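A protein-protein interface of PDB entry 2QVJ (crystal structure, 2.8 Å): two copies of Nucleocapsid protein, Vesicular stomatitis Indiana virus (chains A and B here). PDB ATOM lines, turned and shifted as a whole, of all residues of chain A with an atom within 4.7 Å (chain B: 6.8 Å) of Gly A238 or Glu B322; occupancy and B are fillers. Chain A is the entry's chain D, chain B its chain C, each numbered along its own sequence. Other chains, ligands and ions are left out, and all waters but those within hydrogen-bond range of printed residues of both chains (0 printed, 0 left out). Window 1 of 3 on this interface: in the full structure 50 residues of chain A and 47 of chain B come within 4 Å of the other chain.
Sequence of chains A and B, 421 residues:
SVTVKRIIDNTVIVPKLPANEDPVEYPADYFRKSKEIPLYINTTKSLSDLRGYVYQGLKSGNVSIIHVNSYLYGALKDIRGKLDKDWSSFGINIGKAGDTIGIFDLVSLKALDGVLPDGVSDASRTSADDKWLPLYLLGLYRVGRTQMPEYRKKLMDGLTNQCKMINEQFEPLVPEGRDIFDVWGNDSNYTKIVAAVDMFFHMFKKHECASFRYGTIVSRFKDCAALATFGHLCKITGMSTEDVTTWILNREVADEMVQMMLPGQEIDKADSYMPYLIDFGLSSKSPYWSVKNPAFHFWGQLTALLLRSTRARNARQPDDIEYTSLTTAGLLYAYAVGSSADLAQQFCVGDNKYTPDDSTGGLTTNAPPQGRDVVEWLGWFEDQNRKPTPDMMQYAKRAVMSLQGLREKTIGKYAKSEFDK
O of Cys A234 is in hydrogen-bond range of OG1 of Thr A237 (3.2 Å). The backbone carbonyl oxygen of Tyr B323 sits at hydrogen-bond distance from the side-chain hydroxyl of Thr B327 (2.5 Å). OG1 of Thr A237 sits close to N of Met A239 (3.3 Å). The backbone carbonyl oxygen of Thr A237 sits at hydrogen-bond distance from the guanidinium group of Arg A372 (3.2 Å).
Lys A235 touches Ile B321 (O to C, 3.5 Å). Glu B322 touches Lys A235. Ile B321 touches Ile A236 (O to CD1, 3.4 Å). O of Ile A236 touches CG of Glu B322, 3.6 Å away. Tyr B323 touches Ile A236. CA of Gly A238 touches OE1 of Glu B322, 3.2 Å away.
Hydrophobic or aromatic side chains of chain A that line the printed part of chain B: Ile A236. Along chain A the printed residues that touch a printed residue of chain B span positions 235 to 372. Printed residues of chain B that touch a printed residue of chain A: Asp B320, Ile B321, Glu B322 and Tyr B323. Hydrophobic or aromatic side chains of chain B that line the printed part of chain A: Tyr B323. Among the printed residues, Asp or Glu carboxylates within 4 Å of a Lys or Arg side-chain nitrogen of the other chain: Lys A235 with Asp B320 and Arg A372 with Glu B322.
The side-chain carboxylate (OD2) of Asp B320 is in salt-bridge range of the side-chain amino group (NZ) of Lys A235, at 3.6 Å. OE2 of Glu B322 sits close to O of Thr A237 (3.0 Å). OE2 of Glu B322 lies within salt-bridge range of NH1 of Arg A372.
No position is printed for both chains. Of the 9 pairs that touch across the chains among the printed residues, none has its exchanged pair printed and touching as well.
Of the printed residues of chain B, Gly A238 touches Glu B322 (3.2 Å). Printed residues of chain B within 4 Å of Ile A236: Ile B321 (3.4 Å), Glu B322 (3.6 Å) and Tyr B323 (3.5 Å). Printed residues of chain A within 4 Å of Ile B321: Lys A235 (3.5 Å) and Ile A236 (3.4 Å). Of the printed residues of chain A, Asp B320 touches Lys A235 (3.3 Å). Of the printed residues of chain B, Lys A235 touches Asp B320, Ile B321 and Glu B322. Leu B326 touches none of the printed residues of chain A. The nearest printed residue of chain A that does not touch Glu B322 is Met A239 (5.3 Å).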
ATOM      1  N   CYS A 234      -4.195  23.565  33.899  1.00  0.00           N
ATOM      2  CA  CYS A 234      -2.924  22.898  34.159  1.00  0.00           C
ATOM      3  C   CYS A 234      -2.921  21.485  33.593  1.00  0.00           C
ATOM      4  O   CYS A 234      -1.978  21.081  32.916  1.00  0.00           O
ATOM      5  CB  CYS A 234      -2.629  22.861  35.654  1.00  0.00           C
ATOM      6  SG  CYS A 234      -2.214  24.456  36.350  1.00  0.00           S
ATOM      7  N   LYS A 235      -3.990  20.745  33.870  1.00  0.00           N
ATOM      8  CA  LYS A 235      -4.154  19.388  33.366  1.00  0.00           C
ATOM      9  C   LYS A 235      -4.238  19.370  31.838  1.00  0.00           C
ATOM     10  O   LYS A 235      -3.661  18.492  31.188  1.00  0.00           O
ATOM     11  CB  LYS A 235      -5.404  18.745  33.974  1.00  0.00           C
ATOM     12  CG  LYS A 235      -5.422  18.711  35.495  1.00  0.00           C
ATOM     13  CD  LYS A 235      -6.859  18.744  36.004  1.00  0.00           C
ATOM     14  CE  LYS A 235      -6.951  18.568  37.517  1.00  0.00           C
ATOM     15  NZ  LYS A 235      -8.372  18.493  37.960  1.00  0.00           N
ATOM     16  N   ILE A 236      -4.941  20.352  31.275  1.00  0.00           N
ATOM     17  CA  ILE A 236      -5.156  20.430  29.831  1.00  0.00           C
ATOM     18  C   ILE A 236      -3.857  20.744  29.060  1.00  0.00           C
ATOM     19  O   ILE A 236      -3.672  20.283  27.930  1.00  0.00           O
ATOM     20  CB  ILE A 236      -6.321  21.424  29.483  1.00  0.00           C
ATOM     21  CG1 ILE A 236      -7.371  20.782  28.559  1.00  0.00           C
ATOM     22  CG2 ILE A 236      -5.807  22.775  28.993  1.00  0.00           C
ATOM     23  CD1 ILE A 236      -6.846  20.194  27.283  1.00  0.00           C
ATOM     24  N   THR A 237      -2.962  21.508  29.680  1.00  0.00           N
ATOM     25  CA  THR A 237      -1.676  21.841  29.067  1.00  0.00           C
ATOM     26  C   THR A 237      -0.597  20.833  29.455  1.00  0.00           C
ATOM     27  O   THR A 237       0.425  20.715  28.774  1.00  0.00           O
ATOM     28  CB  THR A 237      -1.189  23.264  29.451  1.00  0.00           C
ATOM     29  OG1 THR A 237      -1.087  23.377  30.876  1.00  0.00           O
ATOM     30  CG2 THR A 237      -2.140  24.330  28.926  1.00  0.00           C
ATOM     31  N   GLY A 238      -0.832  20.112  30.550  1.00  0.00           N
ATOM     32  CA  GLY A 238       0.158  19.195  31.108  1.00  0.00           C
ATOM     33  C   GLY A 238       1.362  19.937  31.654  1.00  0.00           C
ATOM     34  O   GLY A 238       2.465  19.392  31.717  1.00  0.00           O
ATOM     35  N   MET A 239       1.142  21.192  32.040  1.00  0.00           N
ATOM     36  CA  MET A 239       2.193  22.049  32.576  1.00  0.00           C
ATOM     37  C   MET A 239       1.988  22.257  34.070  1.00  0.00           C
ATOM     38  O   MET A 239       0.876  22.114  34.578  1.00  0.00           O
ATOM     39  CB  MET A 239       2.209  23.392  31.848  1.00  0.00           C
ATOM     40  CG  MET A 239       2.661  23.313  30.393  1.00  0.00           C
ATOM     41  SD  MET A 239       2.387  24.837  29.463  1.00  0.00           S
ATOM     42  CE  MET A 239       3.612  25.923  30.194  1.00  0.00           C
ATOM     43  N   SER A 240       3.066  22.588  34.770  1.00  0.00           N
ATOM     44  CA  SER A 240       3.004  22.793  36.212  1.00  0.00           C
ATOM     45  C   SER A 240       2.345  24.126  36.540  1.00  0.00           C
ATOM     46  O   SER A 240       2.261  25.012  35.685  1.00  0.00           O
ATOM     47  CB  SER A 240       4.402  22.729  36.830  1.00  0.00           C
ATOM     48  OG  SER A 240       5.174  23.860  36.468  1.00  0.00           O
ATOM     49  N   ARG A 372       8.059  25.218  24.972  1.00  0.00           N
ATOM     50  CA  ARG A 372       6.864  25.935  25.424  1.00  0.00           C
ATOM     51  C   ARG A 372       7.248  27.054  26.399  1.00  0.00           C
ATOM     52  O   ARG A 372       6.539  27.328  27.371  1.00  0.00           O
ATOM     53  CB  ARG A 372       5.831  24.971  26.034  1.00  0.00           C
ATOM     54  CG  ARG A 372       5.355  23.885  25.067  1.00  0.00           C
ATOM     55  CD  ARG A 372       4.035  23.246  25.477  1.00  0.00           C
ATOM     56  NE  ARG A 372       4.150  22.432  26.684  1.00  0.00           N
ATOM     57  CZ  ARG A 372       3.327  21.436  27.006  1.00  0.00           C
ATOM     58  NH1 ARG A 372       2.324  21.100  26.205  1.00  0.00           N
ATOM     59  NH2 ARG A 372       3.518  20.762  28.131  1.00  0.00           N
ATOM     60  N   ASN B 250       4.416   9.844  26.658  1.00  0.00           N
ATOM     61  CA  ASN B 250       3.994  10.876  27.600  1.00  0.00           C
ATOM     62  C   ASN B 250       4.316  10.468  29.036  1.00  0.00           C
ATOM     63  O   ASN B 250       4.295   9.281  29.363  1.00  0.00           O
ATOM     64  CB  ASN B 250       2.492  11.157  27.462  1.00  0.00           C
ATOM     65  CG  ASN B 250       1.989  11.027  26.025  1.00  0.00           C
ATOM     66  OD1 ASN B 250       1.816  12.026  25.324  1.00  0.00           O
ATOM     67  ND2 ASN B 250       1.747   9.790  25.585  1.00  0.00           N
ATOM     68  N   ARG B 251       4.606  11.454  29.885  1.00  0.00           N
ATOM     69  CA  ARG B 251       4.963  11.222  31.290  1.00  0.00           C
ATOM     70  C   ARG B 251       3.775  10.741  32.133  1.00  0.00           C
ATOM     71  O   ARG B 251       3.941   9.929  33.047  1.00  0.00           O
ATOM     72  CB  ARG B 251       5.563  12.494  31.898  1.00  0.00           C
ATOM     73  CG  ARG B 251       6.128  12.335  33.307  1.00  0.00           C
ATOM     74  CD  ARG B 251       6.628  13.669  33.875  1.00  0.00           C
ATOM     75  NE  ARG B 251       5.541  14.608  34.175  1.00  0.00           N
ATOM     76  CZ  ARG B 251       4.898  14.684  35.341  1.00  0.00           C
ATOM     77  NH1 ARG B 251       5.219  13.875  36.346  1.00  0.00           N
ATOM     78  NH2 ARG B 251       3.926  15.574  35.501  1.00  0.00           N
ATOM     79  N   GLU B 252       2.584  11.250  31.819  1.00  0.00           N
ATOM     80  CA  GLU B 252       1.363  10.884  32.541  1.00  0.00           C
ATOM     81  C   GLU B 252       0.860   9.486  32.177  1.00  0.00           C
ATOM     82  O   GLU B 252       0.316   8.783  33.030  1.00  0.00           O
ATOM     83  CB  GLU B 252       0.260  11.927  32.323  1.00  0.00           C
ATOM     84  CG  GLU B 252       0.434  13.226  33.125  1.00  0.00           C
ATOM     85  CD  GLU B 252       1.312  14.262  32.426  1.00  0.00           C
ATOM     86  OE1 GLU B 252       0.808  15.371  32.141  1.00  0.00           O
ATOM     87  OE2 GLU B 252       2.501  13.977  32.160  1.00  0.00           O
ATOM     88  N   ALA B 295      -5.251   9.193  30.972  1.00  0.00           N
ATOM     89  CA  ALA B 295      -4.268   9.434  29.911  1.00  0.00           C
ATOM     90  C   ALA B 295      -4.055   8.216  29.013  1.00  0.00           C
ATOM     91  O   ALA B 295      -4.007   8.345  27.787  1.00  0.00           O
ATOM     92  CB  ALA B 295      -2.944   9.915  30.501  1.00  0.00           C
ATOM     93  N   PHE B 298      -7.243   7.302  26.871  1.00  0.00           N
ATOM     94  CA  PHE B 298      -7.313   8.114  25.664  1.00  0.00           C
ATOM     95  C   PHE B 298      -6.272   7.650  24.646  1.00  0.00           C
ATOM     96  O   PHE B 298      -6.615   7.325  23.509  1.00  0.00           O
ATOM     97  CB  PHE B 298      -7.117   9.594  26.008  1.00  0.00           C
ATOM     98  CG  PHE B 298      -7.289  10.524  24.837  1.00  0.00           C
ATOM     99  CD1 PHE B 298      -8.535  11.067  24.543  1.00  0.00           C
ATOM    100  CD2 PHE B 298      -6.205  10.864  24.036  1.00  0.00           C
ATOM    101  CE1 PHE B 298      -8.702  11.927  23.462  1.00  0.00           C
ATOM    102  CE2 PHE B 298      -6.363  11.722  22.951  1.00  0.00           C
ATOM    103  CZ  PHE B 298      -7.616  12.255  22.666  1.00  0.00           C
ATOM    104  N   ASP B 319     -12.007  13.876  30.411  1.00  0.00           N
ATOM    105  CA  ASP B 319     -11.422  15.217  30.436  1.00  0.00           C
ATOM    106  C   ASP B 319     -10.317  15.340  31.484  1.00  0.00           C
ATOM    107  O   ASP B 319      -9.967  14.356  32.137  1.00  0.00           O
ATOM    108  CB  ASP B 319     -12.483  16.332  30.554  1.00  0.00           C
ATOM    109  CG  ASP B 319     -13.478  16.101  31.678  1.00  0.00           C
ATOM    110  OD1 ASP B 319     -13.060  15.726  32.795  1.00  0.00           O
ATOM    111  OD2 ASP B 319     -14.685  16.325  31.441  1.00  0.00           O
ATOM    112  N   ASP B 320      -9.767  16.546  31.615  1.00  0.00           N
ATOM    113  CA  ASP B 320      -8.634  16.837  32.504  1.00  0.00           C
ATOM    114  C   ASP B 320      -7.339  16.126  32.098  1.00  0.00           C
ATOM    115  O   ASP B 320      -6.504  15.795  32.944  1.00  0.00           O
ATOM    116  CB  ASP B 320      -8.992  16.584  33.977  1.00  0.00           C
ATOM    117  CG  ASP B 320      -9.961  17.620  34.531  1.00  0.00           C
ATOM    118  OD1 ASP B 320      -9.988  18.762  34.020  1.00  0.00           O
ATOM    119  OD2 ASP B 320     -10.692  17.290  35.491  1.00  0.00           O
ATOM    120  N   ILE B 321      -7.181  15.902  30.795  1.00  0.00           N
ATOM    121  CA  ILE B 321      -5.936  15.365  30.237  1.00  0.00           C
ATOM    122  C   ILE B 321      -5.380  16.273  29.142  1.00  0.00           C
ATOM    123  O   ILE B 321      -5.999  17.273  28.782  1.00  0.00           O
ATOM    124  CB  ILE B 321      -6.099  13.918  29.699  1.00  0.00           C
ATOM    125  CG1 ILE B 321      -7.246  13.833  28.685  1.00  0.00           C
ATOM    126  CG2 ILE B 321      -6.289  12.940  30.851  1.00  0.00           C
ATOM    127  CD1 ILE B 321      -7.235  12.577  27.842  1.00  0.00           C
ATOM    128  N   GLU B 322      -4.211  15.916  28.624  1.00  0.00           N
ATOM    129  CA  GLU B 322      -3.548  16.693  27.589  1.00  0.00           C
ATOM    130  C   GLU B 322      -3.903  16.112  26.224  1.00  0.00           C
ATOM    131  O   GLU B 322      -3.192  15.258  25.703  1.00  0.00           O
ATOM    132  CB  GLU B 322      -2.039  16.661  27.817  1.00  0.00           C
ATOM    133  CG  GLU B 322      -1.266  17.781  27.148  1.00  0.00           C
ATOM    134  CD  GLU B 322       0.192  17.801  27.570  1.00  0.00           C
ATOM    135  OE1 GLU B 322       0.517  17.175  28.599  1.00  0.00           O
ATOM    136  OE2 GLU B 322       1.010  18.440  26.873  1.00  0.00           O
ATOM    137  N   TYR B 323      -5.014  16.582  25.659  1.00  0.00           N
ATOM    138  CA  TYR B 323      -5.547  16.042  24.407  1.00  0.00           C
ATOM    139  C   TYR B 323      -4.569  16.139  23.246  1.00  0.00           C
ATOM    140  O   TYR B 323      -4.349  15.158  22.540  1.00  0.00           O
ATOM    141  CB  TYR B 323      -6.847  16.746  24.021  1.00  0.00           C
ATOM    142  CG  TYR B 323      -8.002  16.513  24.963  1.00  0.00           C
ATOM    143  CD1 TYR B 323      -8.646  15.276  25.021  1.00  0.00           C
ATOM    144  CD2 TYR B 323      -8.470  17.537  25.778  1.00  0.00           C
ATOM    145  CE1 TYR B 323      -9.712  15.066  25.878  1.00  0.00           C
ATOM    146  CE2 TYR B 323      -9.537  17.339  26.637  1.00  0.00           C
ATOM    147  CZ  TYR B 323     -10.152  16.103  26.682  1.00  0.00           C
ATOM    148  OH  TYR B 323     -11.209  15.910  27.532  1.00  0.00           O
ATOM    149  N   THR B 324      -3.989  17.324  23.059  1.00  0.00           N
ATOM    150  CA  THR B 324      -3.126  17.620  21.914  1.00  0.00           C
ATOM    151  C   THR B 324      -1.894  16.724  21.848  1.00  0.00           C
ATOM    152  O   THR B 324      -1.589  16.154  20.799  1.00  0.00           O
ATOM    153  CB  THR B 324      -2.656  19.092  21.933  1.00  0.00           C
ATOM    154  OG1 THR B 324      -1.988  19.366  23.172  1.00  0.00           O
ATOM    155  CG2 THR B 324      -3.838  20.040  21.769  1.00  0.00           C
ATOM    156  N   SER B 325      -1.199  16.607  22.977  1.00  0.00           N
ATOM    157  CA  SER B 325       0.050  15.855  23.067  1.00  0.00           C
ATOM    158  C   SER B 325      -0.180  14.348  22.951  1.00  0.00           C
ATOM    159  O   SER B 325       0.610  13.633  22.333  1.00  0.00           O
ATOM    160  CB  SER B 325       0.756  16.187  24.382  1.00  0.00           C
ATOM    161  OG  SER B 325       2.099  15.746  24.366  1.00  0.00           O
ATOM    162  N   LEU B 326      -1.272  13.882  23.550  1.00  0.00           N
ATOM    163  CA  LEU B 326      -1.663  12.477  23.492  1.00  0.00           C
ATOM    164  C   LEU B 326      -2.134  12.099  22.093  1.00  0.00           C
ATOM    165  O   LEU B 326      -1.960  10.955  21.665  1.00  0.00           O
ATOM    166  CB  LEU B 326      -2.763  12.184  24.516  1.00  0.00           C
ATOM    167  CG  LEU B 326      -2.417  11.780  25.959  1.00  0.00           C
ATOM    168  CD1 LEU B 326      -1.417  12.709  26.633  1.00  0.00           C
ATOM    169  CD2 LEU B 326      -3.685  11.698  26.791  1.00  0.00           C
ATOM    170  N   THR B 327      -2.725  13.063  21.389  1.00  0.00           N
ATOM    171  CA  THR B 327      -3.200  12.860  20.024  1.00  0.00           C
ATOM    172  C   THR B 327      -2.035  12.606  19.065  1.00  0.00           C
ATOM    173  O   THR B 327      -2.035  11.614  18.332  1.00  0.00           O
ATOM    174  CB  THR B 327      -4.049  14.057  19.538  1.00  0.00           C
ATOM    175  OG1 THR B 327      -5.214  14.182  20.361  1.00  0.00           O
ATOM    176  CG2 THR B 327      -4.482  13.873  18.090  1.00  0.00           C
